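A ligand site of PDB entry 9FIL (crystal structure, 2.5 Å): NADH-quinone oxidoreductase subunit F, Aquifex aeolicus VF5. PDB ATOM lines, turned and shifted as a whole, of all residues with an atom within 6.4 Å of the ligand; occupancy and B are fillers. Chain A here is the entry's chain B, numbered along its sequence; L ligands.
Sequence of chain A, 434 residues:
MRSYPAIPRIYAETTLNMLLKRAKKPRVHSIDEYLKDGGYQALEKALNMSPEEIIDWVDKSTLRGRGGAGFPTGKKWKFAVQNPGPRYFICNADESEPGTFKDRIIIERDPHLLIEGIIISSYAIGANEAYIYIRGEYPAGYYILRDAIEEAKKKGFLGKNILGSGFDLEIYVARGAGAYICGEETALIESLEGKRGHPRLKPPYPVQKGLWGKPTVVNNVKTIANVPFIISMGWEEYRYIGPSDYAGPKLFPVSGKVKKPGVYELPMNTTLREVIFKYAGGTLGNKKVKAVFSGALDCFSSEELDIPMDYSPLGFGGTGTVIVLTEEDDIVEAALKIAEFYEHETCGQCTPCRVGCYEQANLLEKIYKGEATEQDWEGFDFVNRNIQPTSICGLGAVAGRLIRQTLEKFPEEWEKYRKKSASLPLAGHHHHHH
A sulfur (S3) of the ligand sits close to the backbone NH (N) of Cys 350 (3.2 Å).
SG of Cys 350 is bound to FE4 of the ligand (2.2 Å).
The side-chain sulfur (SG) of Cys 353 binds an iron atom (FE2) of the ligand (2.3 Å).
N of Cys 347 sits close to S4 of the ligand, 3.7 Å away.
SG of Cys 347 binds FE1 of the ligand, 2.3 Å away.
An iron atom (FE3) of the ligand is bound by the side-chain sulfur (SG) of Cys 393, at 2.3 Å.
The backbone NH (N) of Gln 349 sits close to a sulfur (S3) of the ligand (3.3 Å).
NE2 of Gln 349 sits close to S2 of the ligand, 3.5 Å away.
A sulfur (S1) of the ligand sits close to the backbone NH of Gly 396, at 3.6 Å.
The backbone NH (N) of Gly 348 sits close to a sulfur (S3) of the ligand (3.6 Å).
A sulfur (S3) of the ligand lies close to the side-chain hydroxyl (OG1) of Thr 346 (3.8 Å).
SG of Cys 350 sits close to N of Ile 392 (3.3 Å).
SG of Cys 353 lies close to OG1 of Thr 346, at 3.1 Å.
The backbone carbonyl oxygen (O) of Cys 353 sits close to the side-chain sulfur (SG) of Cys 357, at 3.4 Å.
N of Cys 353 is in hydrogen-bond range of O of Ile 387 (3.4 Å).
The side-chain sulfur (SG) of Cys 347 sits close to the side-chain amide nitrogen (NE2) of Gln 349, at 3.6 Å.
The backbone NH (N) of Leu 395 lies close to the side-chain sulfur (SG) of Cys 393, at 3.5 Å.
NE2 of Gln 349 sits at hydrogen-bond distance from O of Pro 199.
The backbone NH (N) of Gly 348 lies within hydrogen-bond range of the side-chain hydroxyl (OG1) of Thr 346 (3.4 Å).
Residues that only touch the ligand: Ile 181 (3.6 Å), Pro 199 (3.7 Å), Ser 391 (3.6 Å), Ile 392 (3.3 Å) and Leu 395 (3.8 Å).
Hydrophobic or aromatic side chains that line the ligand: Ile 181, Pro 199, Ile 392 and Leu 395.
Within 4 Å of the ligand: Ile 181, Pro 199, Thr 346, Cys 347, Gly 348, Gln 349, Cys 350, Cys 353, Ser 391, Ile 392, Cys 393, Leu 395 and Gly 396.
The nearest printed residue that does not touch the ligand is Glu 345 (4.7 Å).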
ATOM      1  N   ILE A 181       2.561  -8.939 -21.741  1.00  0.00           N
ATOM      2  CA  ILE A 181       3.102  -8.663 -23.067  1.00  0.00           C
ATOM      3  C   ILE A 181       2.569  -9.684 -24.078  1.00  0.00           C
ATOM      4  O   ILE A 181       2.390  -9.340 -25.234  1.00  0.00           O
ATOM      5  CB  ILE A 181       4.645  -8.607 -23.022  1.00  0.00           C
ATOM      6  CG1 ILE A 181       5.214  -7.835 -24.215  1.00  0.00           C
ATOM      7  CG2 ILE A 181       5.278 -10.002 -22.910  1.00  0.00           C
ATOM      8  CD1 ILE A 181       4.579  -6.486 -24.443  1.00  0.00           C
ATOM      9  N   GLY A 197       7.793 -14.405 -24.842  1.00  0.00           N
ATOM     10  CA  GLY A 197       6.832 -13.478 -25.422  1.00  0.00           C
ATOM     11  C   GLY A 197       7.494 -12.141 -25.742  1.00  0.00           C
ATOM     12  O   GLY A 197       7.136 -11.140 -25.141  1.00  0.00           O
ATOM     13  N   HIS A 198       8.445 -12.148 -26.676  1.00  0.00           N
ATOM     14  CA  HIS A 198       9.070 -10.914 -27.108  1.00  0.00           C
ATOM     15  C   HIS A 198       8.366 -10.391 -28.350  1.00  0.00           C
ATOM     16  O   HIS A 198       8.343 -11.063 -29.379  1.00  0.00           O
ATOM     17  CB  HIS A 198      10.579 -11.117 -27.341  1.00  0.00           C
ATOM     18  CG  HIS A 198      11.314 -11.308 -26.053  1.00  0.00           C
ATOM     19  ND1 HIS A 198      12.465 -12.049 -25.924  1.00  0.00           N
ATOM     20  CD2 HIS A 198      11.043 -10.829 -24.823  1.00  0.00           C
ATOM     21  CE1 HIS A 198      12.868 -12.018 -24.654  1.00  0.00           C
ATOM     22  NE2 HIS A 198      12.004 -11.288 -23.963  1.00  0.00           N
ATOM     23  N   PRO A 199       7.771  -9.172 -28.301  1.00  0.00           N
ATOM     24  CA  PRO A 199       7.220  -8.539 -29.504  1.00  0.00           C
ATOM     25  C   PRO A 199       8.205  -8.365 -30.656  1.00  0.00           C
ATOM     26  O   PRO A 199       9.378  -8.017 -30.429  1.00  0.00           O
ATOM     27  CB  PRO A 199       6.770  -7.172 -28.956  1.00  0.00           C
ATOM     28  CG  PRO A 199       6.447  -7.455 -27.499  1.00  0.00           C
ATOM     29  CD  PRO A 199       7.602  -8.345 -27.103  1.00  0.00           C
ATOM     30  N   ARG A 200       7.691  -8.584 -31.880  1.00  0.00           N
ATOM     31  CA  ARG A 200       8.401  -8.322 -33.133  1.00  0.00           C
ATOM     32  C   ARG A 200       8.178  -6.889 -33.584  1.00  0.00           C
ATOM     33  O   ARG A 200       7.113  -6.326 -33.381  1.00  0.00           O
ATOM     34  CB  ARG A 200       7.858  -9.193 -34.268  1.00  0.00           C
ATOM     35  CG  ARG A 200       7.876 -10.686 -34.011  1.00  0.00           C
ATOM     36  CD  ARG A 200       7.195 -11.418 -35.160  1.00  0.00           C
ATOM     37  NE  ARG A 200       7.046 -12.851 -34.860  1.00  0.00           N
ATOM     38  CZ  ARG A 200       6.415 -13.755 -35.618  1.00  0.00           C
ATOM     39  NH1 ARG A 200       5.735 -13.363 -36.683  1.00  0.00           N
ATOM     40  NH2 ARG A 200       6.494 -15.044 -35.332  1.00  0.00           N
ATOM     41  N   GLU A 345       6.091  -6.089 -16.166  1.00  0.00           N
ATOM     42  CA  GLU A 345       5.551  -6.555 -17.442  1.00  0.00           C
ATOM     43  C   GLU A 345       6.412  -6.177 -18.648  1.00  0.00           C
ATOM     44  O   GLU A 345       6.140  -6.716 -19.727  1.00  0.00           O
ATOM     45  CB  GLU A 345       4.110  -6.083 -17.636  1.00  0.00           C
ATOM     46  CG  GLU A 345       3.125  -6.551 -16.559  1.00  0.00           C
ATOM     47  CD  GLU A 345       3.005  -8.062 -16.360  1.00  0.00           C
ATOM     48  OE1 GLU A 345       3.678  -8.852 -17.058  1.00  0.00           O
ATOM     49  OE2 GLU A 345       2.200  -8.475 -15.507  1.00  0.00           O
ATOM     50  N   THR A 346       7.407  -5.285 -18.525  1.00  0.00           N
ATOM     51  CA  THR A 346       8.314  -5.001 -19.634  1.00  0.00           C
ATOM     52  C   THR A 346       9.058  -6.295 -19.952  1.00  0.00           C
ATOM     53  O   THR A 346       9.442  -7.000 -19.010  1.00  0.00           O
ATOM     54  CB  THR A 346       9.274  -3.852 -19.334  1.00  0.00           C
ATOM     55  OG1 THR A 346      10.166  -3.719 -20.434  1.00  0.00           O
ATOM     56  CG2 THR A 346      10.111  -4.063 -18.080  1.00  0.00           C
ATOM     57  N   CYS A 347       9.228  -6.580 -21.259  1.00  0.00           N
ATOM     58  CA  CYS A 347       9.943  -7.763 -21.728  1.00  0.00           C
ATOM     59  C   CYS A 347      11.459  -7.547 -21.732  1.00  0.00           C
ATOM     60  O   CYS A 347      12.193  -8.525 -21.661  1.00  0.00           O
ATOM     61  CB  CYS A 347       9.371  -8.252 -23.058  1.00  0.00           C
ATOM     62  SG  CYS A 347       9.918  -7.379 -24.540  1.00  0.00           S
ATOM     63  N   GLY A 348      11.940  -6.297 -21.821  1.00  0.00           N
ATOM     64  CA  GLY A 348      13.360  -5.965 -21.644  1.00  0.00           C
ATOM     65  C   GLY A 348      14.125  -5.770 -22.961  1.00  0.00           C
ATOM     66  O   GLY A 348      15.329  -5.463 -22.943  1.00  0.00           O
ATOM     67  N   GLN A 349      13.427  -5.912 -24.109  1.00  0.00           N
ATOM     68  CA  GLN A 349      14.032  -5.843 -25.432  1.00  0.00           C
ATOM     69  C   GLN A 349      14.579  -4.445 -25.710  1.00  0.00           C
ATOM     70  O   GLN A 349      15.700  -4.280 -26.191  1.00  0.00           O
ATOM     71  CB  GLN A 349      12.984  -6.151 -26.496  1.00  0.00           C
ATOM     72  CG  GLN A 349      12.852  -7.628 -26.808  1.00  0.00           C
ATOM     73  CD  GLN A 349      12.082  -7.896 -28.087  1.00  0.00           C
ATOM     74  OE1 GLN A 349      12.697  -8.263 -29.087  1.00  0.00           O
ATOM     75  NE2 GLN A 349      10.768  -7.688 -28.066  1.00  0.00           N
ATOM     76  N   CYS A 350      13.739  -3.433 -25.464  1.00  0.00           N
ATOM     77  CA  CYS A 350      14.088  -2.044 -25.712  1.00  0.00           C
ATOM     78  C   CYS A 350      14.703  -1.519 -24.419  1.00  0.00           C
ATOM     79  O   CYS A 350      14.225  -1.898 -23.351  1.00  0.00           O
ATOM     80  CB  CYS A 350      12.849  -1.278 -26.194  1.00  0.00           C
ATOM     81  SG  CYS A 350      11.747  -2.174 -27.351  1.00  0.00           S
ATOM     82  N   THR A 351      15.761  -0.706 -24.485  1.00  0.00           N
ATOM     83  CA  THR A 351      16.499  -0.327 -23.286  1.00  0.00           C
ATOM     84  C   THR A 351      15.727   0.731 -22.494  1.00  0.00           C
ATOM     85  O   THR A 351      15.556   0.596 -21.279  1.00  0.00           O
ATOM     86  CB  THR A 351      17.919   0.105 -23.674  1.00  0.00           C
ATOM     87  OG1 THR A 351      18.680  -1.089 -23.894  1.00  0.00           O
ATOM     88  CG2 THR A 351      18.627   0.928 -22.601  1.00  0.00           C
ATOM     89  N   CYS A 353      12.578   1.276 -22.224  1.00  0.00           N
ATOM     90  CA  CYS A 353      11.448   0.591 -21.601  1.00  0.00           C
ATOM     91  C   CYS A 353      11.940  -0.253 -20.421  1.00  0.00           C
ATOM     92  O   CYS A 353      11.418  -0.125 -19.316  1.00  0.00           O
ATOM     93  CB  CYS A 353      10.671  -0.179 -22.677  1.00  0.00           C
ATOM     94  SG  CYS A 353       9.326  -1.243 -22.091  1.00  0.00           S
ATOM     95  N   ARG A 354      12.966  -1.087 -20.653  1.00  0.00           N
ATOM     96  CA  ARG A 354      13.489  -1.974 -19.632  1.00  0.00           C
ATOM     97  C   ARG A 354      13.873  -1.176 -18.379  1.00  0.00           C
ATOM     98  O   ARG A 354      13.423  -1.514 -17.281  1.00  0.00           O
ATOM     99  CB  ARG A 354      14.681  -2.765 -20.168  1.00  0.00           C
ATOM    100  CG  ARG A 354      15.403  -3.653 -19.159  1.00  0.00           C
ATOM    101  CD  ARG A 354      16.627  -4.339 -19.756  1.00  0.00           C
ATOM    102  NE  ARG A 354      17.698  -3.422 -20.190  1.00  0.00           N
ATOM    103  CZ  ARG A 354      18.080  -3.248 -21.453  1.00  0.00           C
ATOM    104  NH1 ARG A 354      17.392  -3.773 -22.471  1.00  0.00           N
ATOM    105  NH2 ARG A 354      19.148  -2.508 -21.712  1.00  0.00           N
ATOM    106  N   CYS A 357      10.755   1.504 -16.983  1.00  0.00           N
ATOM    107  CA  CYS A 357       9.694   0.879 -16.199  1.00  0.00           C
ATOM    108  C   CYS A 357      10.230   0.509 -14.818  1.00  0.00           C
ATOM    109  O   CYS A 357       9.524   0.664 -13.812  1.00  0.00           O
ATOM    110  CB  CYS A 357       9.067  -0.311 -16.916  1.00  0.00           C
ATOM    111  SG  CYS A 357       8.171   0.121 -18.437  1.00  0.00           S
ATOM    112  N   ILE A 387      10.521   6.632 -21.435  1.00  0.00           N
ATOM    113  CA  ILE A 387      10.358   5.187 -21.496  1.00  0.00           C
ATOM    114  C   ILE A 387      10.070   4.773 -22.940  1.00  0.00           C
ATOM    115  O   ILE A 387      10.397   3.647 -23.334  1.00  0.00           O
ATOM    116  CB  ILE A 387       9.249   4.695 -20.544  1.00  0.00           C
ATOM    117  CG1 ILE A 387       9.305   5.419 -19.175  1.00  0.00           C
ATOM    118  CG2 ILE A 387       9.311   3.177 -20.393  1.00  0.00           C
ATOM    119  CD1 ILE A 387       8.328   4.900 -18.137  1.00  0.00           C
ATOM    120  N   THR A 390      12.735   4.423 -28.897  1.00  0.00           N
ATOM    121  CA  THR A 390      13.210   3.185 -29.522  1.00  0.00           C
ATOM    122  C   THR A 390      12.289   1.977 -29.251  1.00  0.00           C
ATOM    123  O   THR A 390      12.601   0.867 -29.670  1.00  0.00           O
ATOM    124  CB  THR A 390      14.661   2.859 -29.129  1.00  0.00           C
ATOM    125  OG1 THR A 390      14.726   2.390 -27.785  1.00  0.00           O
ATOM    126  CG2 THR A 390      15.598   4.039 -29.304  1.00  0.00           C
ATOM    127  N   SER A 391      11.142   2.177 -28.588  1.00  0.00           N
ATOM    128  CA  SER A 391      10.269   1.073 -28.227  1.00  0.00           C
ATOM    129  C   SER A 391       9.629   0.420 -29.442  1.00  0.00           C
ATOM    130  O   SER A 391       9.143   1.105 -30.335  1.00  0.00           O
ATOM    131  CB  SER A 391       9.192   1.548 -27.263  1.00  0.00           C
ATOM    132  OG  SER A 391       8.324   2.512 -27.845  1.00  0.00           O
ATOM    133  N   ILE A 392       9.568  -0.922 -29.472  1.00  0.00           N
ATOM    134  CA  ILE A 392       9.004  -1.626 -30.612  1.00  0.00           C
ATOM    135  C   ILE A 392       7.536  -2.024 -30.368  1.00  0.00           C
ATOM    136  O   ILE A 392       6.882  -2.432 -31.308  1.00  0.00           O
ATOM    137  CB  ILE A 392       9.872  -2.836 -31.038  1.00  0.00           C
ATOM    138  CG1 ILE A 392       9.939  -3.944 -29.985  1.00  0.00           C
ATOM    139  CG2 ILE A 392      11.289  -2.391 -31.423  1.00  0.00           C
ATOM    140  CD1 ILE A 392      10.928  -5.053 -30.302  1.00  0.00           C
ATOM    141  N   CYS A 393       7.006  -1.919 -29.152  1.00  0.00           N
ATOM    142  CA  CYS A 393       5.570  -2.150 -28.936  1.00  0.00           C
ATOM    143  C   CYS A 393       4.984  -1.018 -28.098  1.00  0.00           C
ATOM    144  O   CYS A 393       5.692  -0.075 -27.737  1.00  0.00           O
ATOM    145  CB  CYS A 393       5.233  -3.518 -28.347  1.00  0.00           C
ATOM    146  SG  CYS A 393       5.290  -3.617 -26.540  1.00  0.00           S
ATOM    147  N   GLY A 394       3.669  -1.137 -27.828  1.00  0.00           N
ATOM    148  CA  GLY A 394       2.852  -0.074 -27.256  1.00  0.00           C
ATOM    149  C   GLY A 394       2.982   0.065 -25.745  1.00  0.00           C
ATOM    150  O   GLY A 394       2.640   1.119 -25.199  1.00  0.00           O
ATOM    151  N   LEU A 395       3.503  -0.975 -25.076  1.00  0.00           N
ATOM    152  CA  LEU A 395       3.778  -0.923 -23.655  1.00  0.00           C
ATOM    153  C   LEU A 395       4.695   0.263 -23.340  1.00  0.00           C
ATOM    154  O   LEU A 395       4.335   1.147 -22.567  1.00  0.00           O
ATOM    155  CB  LEU A 395       4.382  -2.238 -23.140  1.00  0.00           C
ATOM    156  CG  LEU A 395       4.420  -2.410 -21.619  1.00  0.00           C
ATOM    157  CD1 LEU A 395       4.242  -3.862 -21.228  1.00  0.00           C
ATOM    158  CD2 LEU A 395       5.707  -1.878 -20.971  1.00  0.00           C
ATOM    159  N   GLY A 396       5.870   0.270 -23.973  1.00  0.00           N
ATOM    160  CA  GLY A 396       6.860   1.299 -23.746  1.00  0.00           C
ATOM    161  C   GLY A 396       6.335   2.658 -24.198  1.00  0.00           C
ATOM    162  O   GLY A 396       6.822   3.692 -23.730  1.00  0.00           O
ATOM    163  N   ALA A 397       5.349   2.635 -25.103  1.00  0.00           N
ATOM    164  CA  ALA A 397       4.749   3.868 -25.576  1.00  0.00           C
ATOM    165  C   ALA A 397       3.861   4.462 -24.486  1.00  0.00           C
ATOM    166  O   ALA A 397       3.791   5.677 -24.405  1.00  0.00           O
ATOM    167  CB  ALA A 397       4.003   3.665 -26.879  1.00  0.00           C
HETATM  168 FE1  LIG L   1       9.302  -5.200 -24.659  1.00  0.00          FE
HETATM  169 FE2  LIG L   1       8.888  -2.725 -23.728  1.00  0.00          FE
HETATM  170 FE3  LIG L   1       7.450  -3.604 -25.818  1.00  0.00          FE
HETATM  171 FE4  LIG L   1      10.116  -3.106 -26.117  1.00  0.00          FE
HETATM  172  S1  LIG L   1       8.428  -1.597 -25.633  1.00  0.00           S
HETATM  173  S2  LIG L   1       8.985  -4.885 -26.925  1.00  0.00           S
HETATM  174  S3  LIG L   1      10.900  -3.741 -24.113  1.00  0.00           S
HETATM  175  S4  LIG L   1       7.437  -4.425 -23.667  1.00  0.00           S
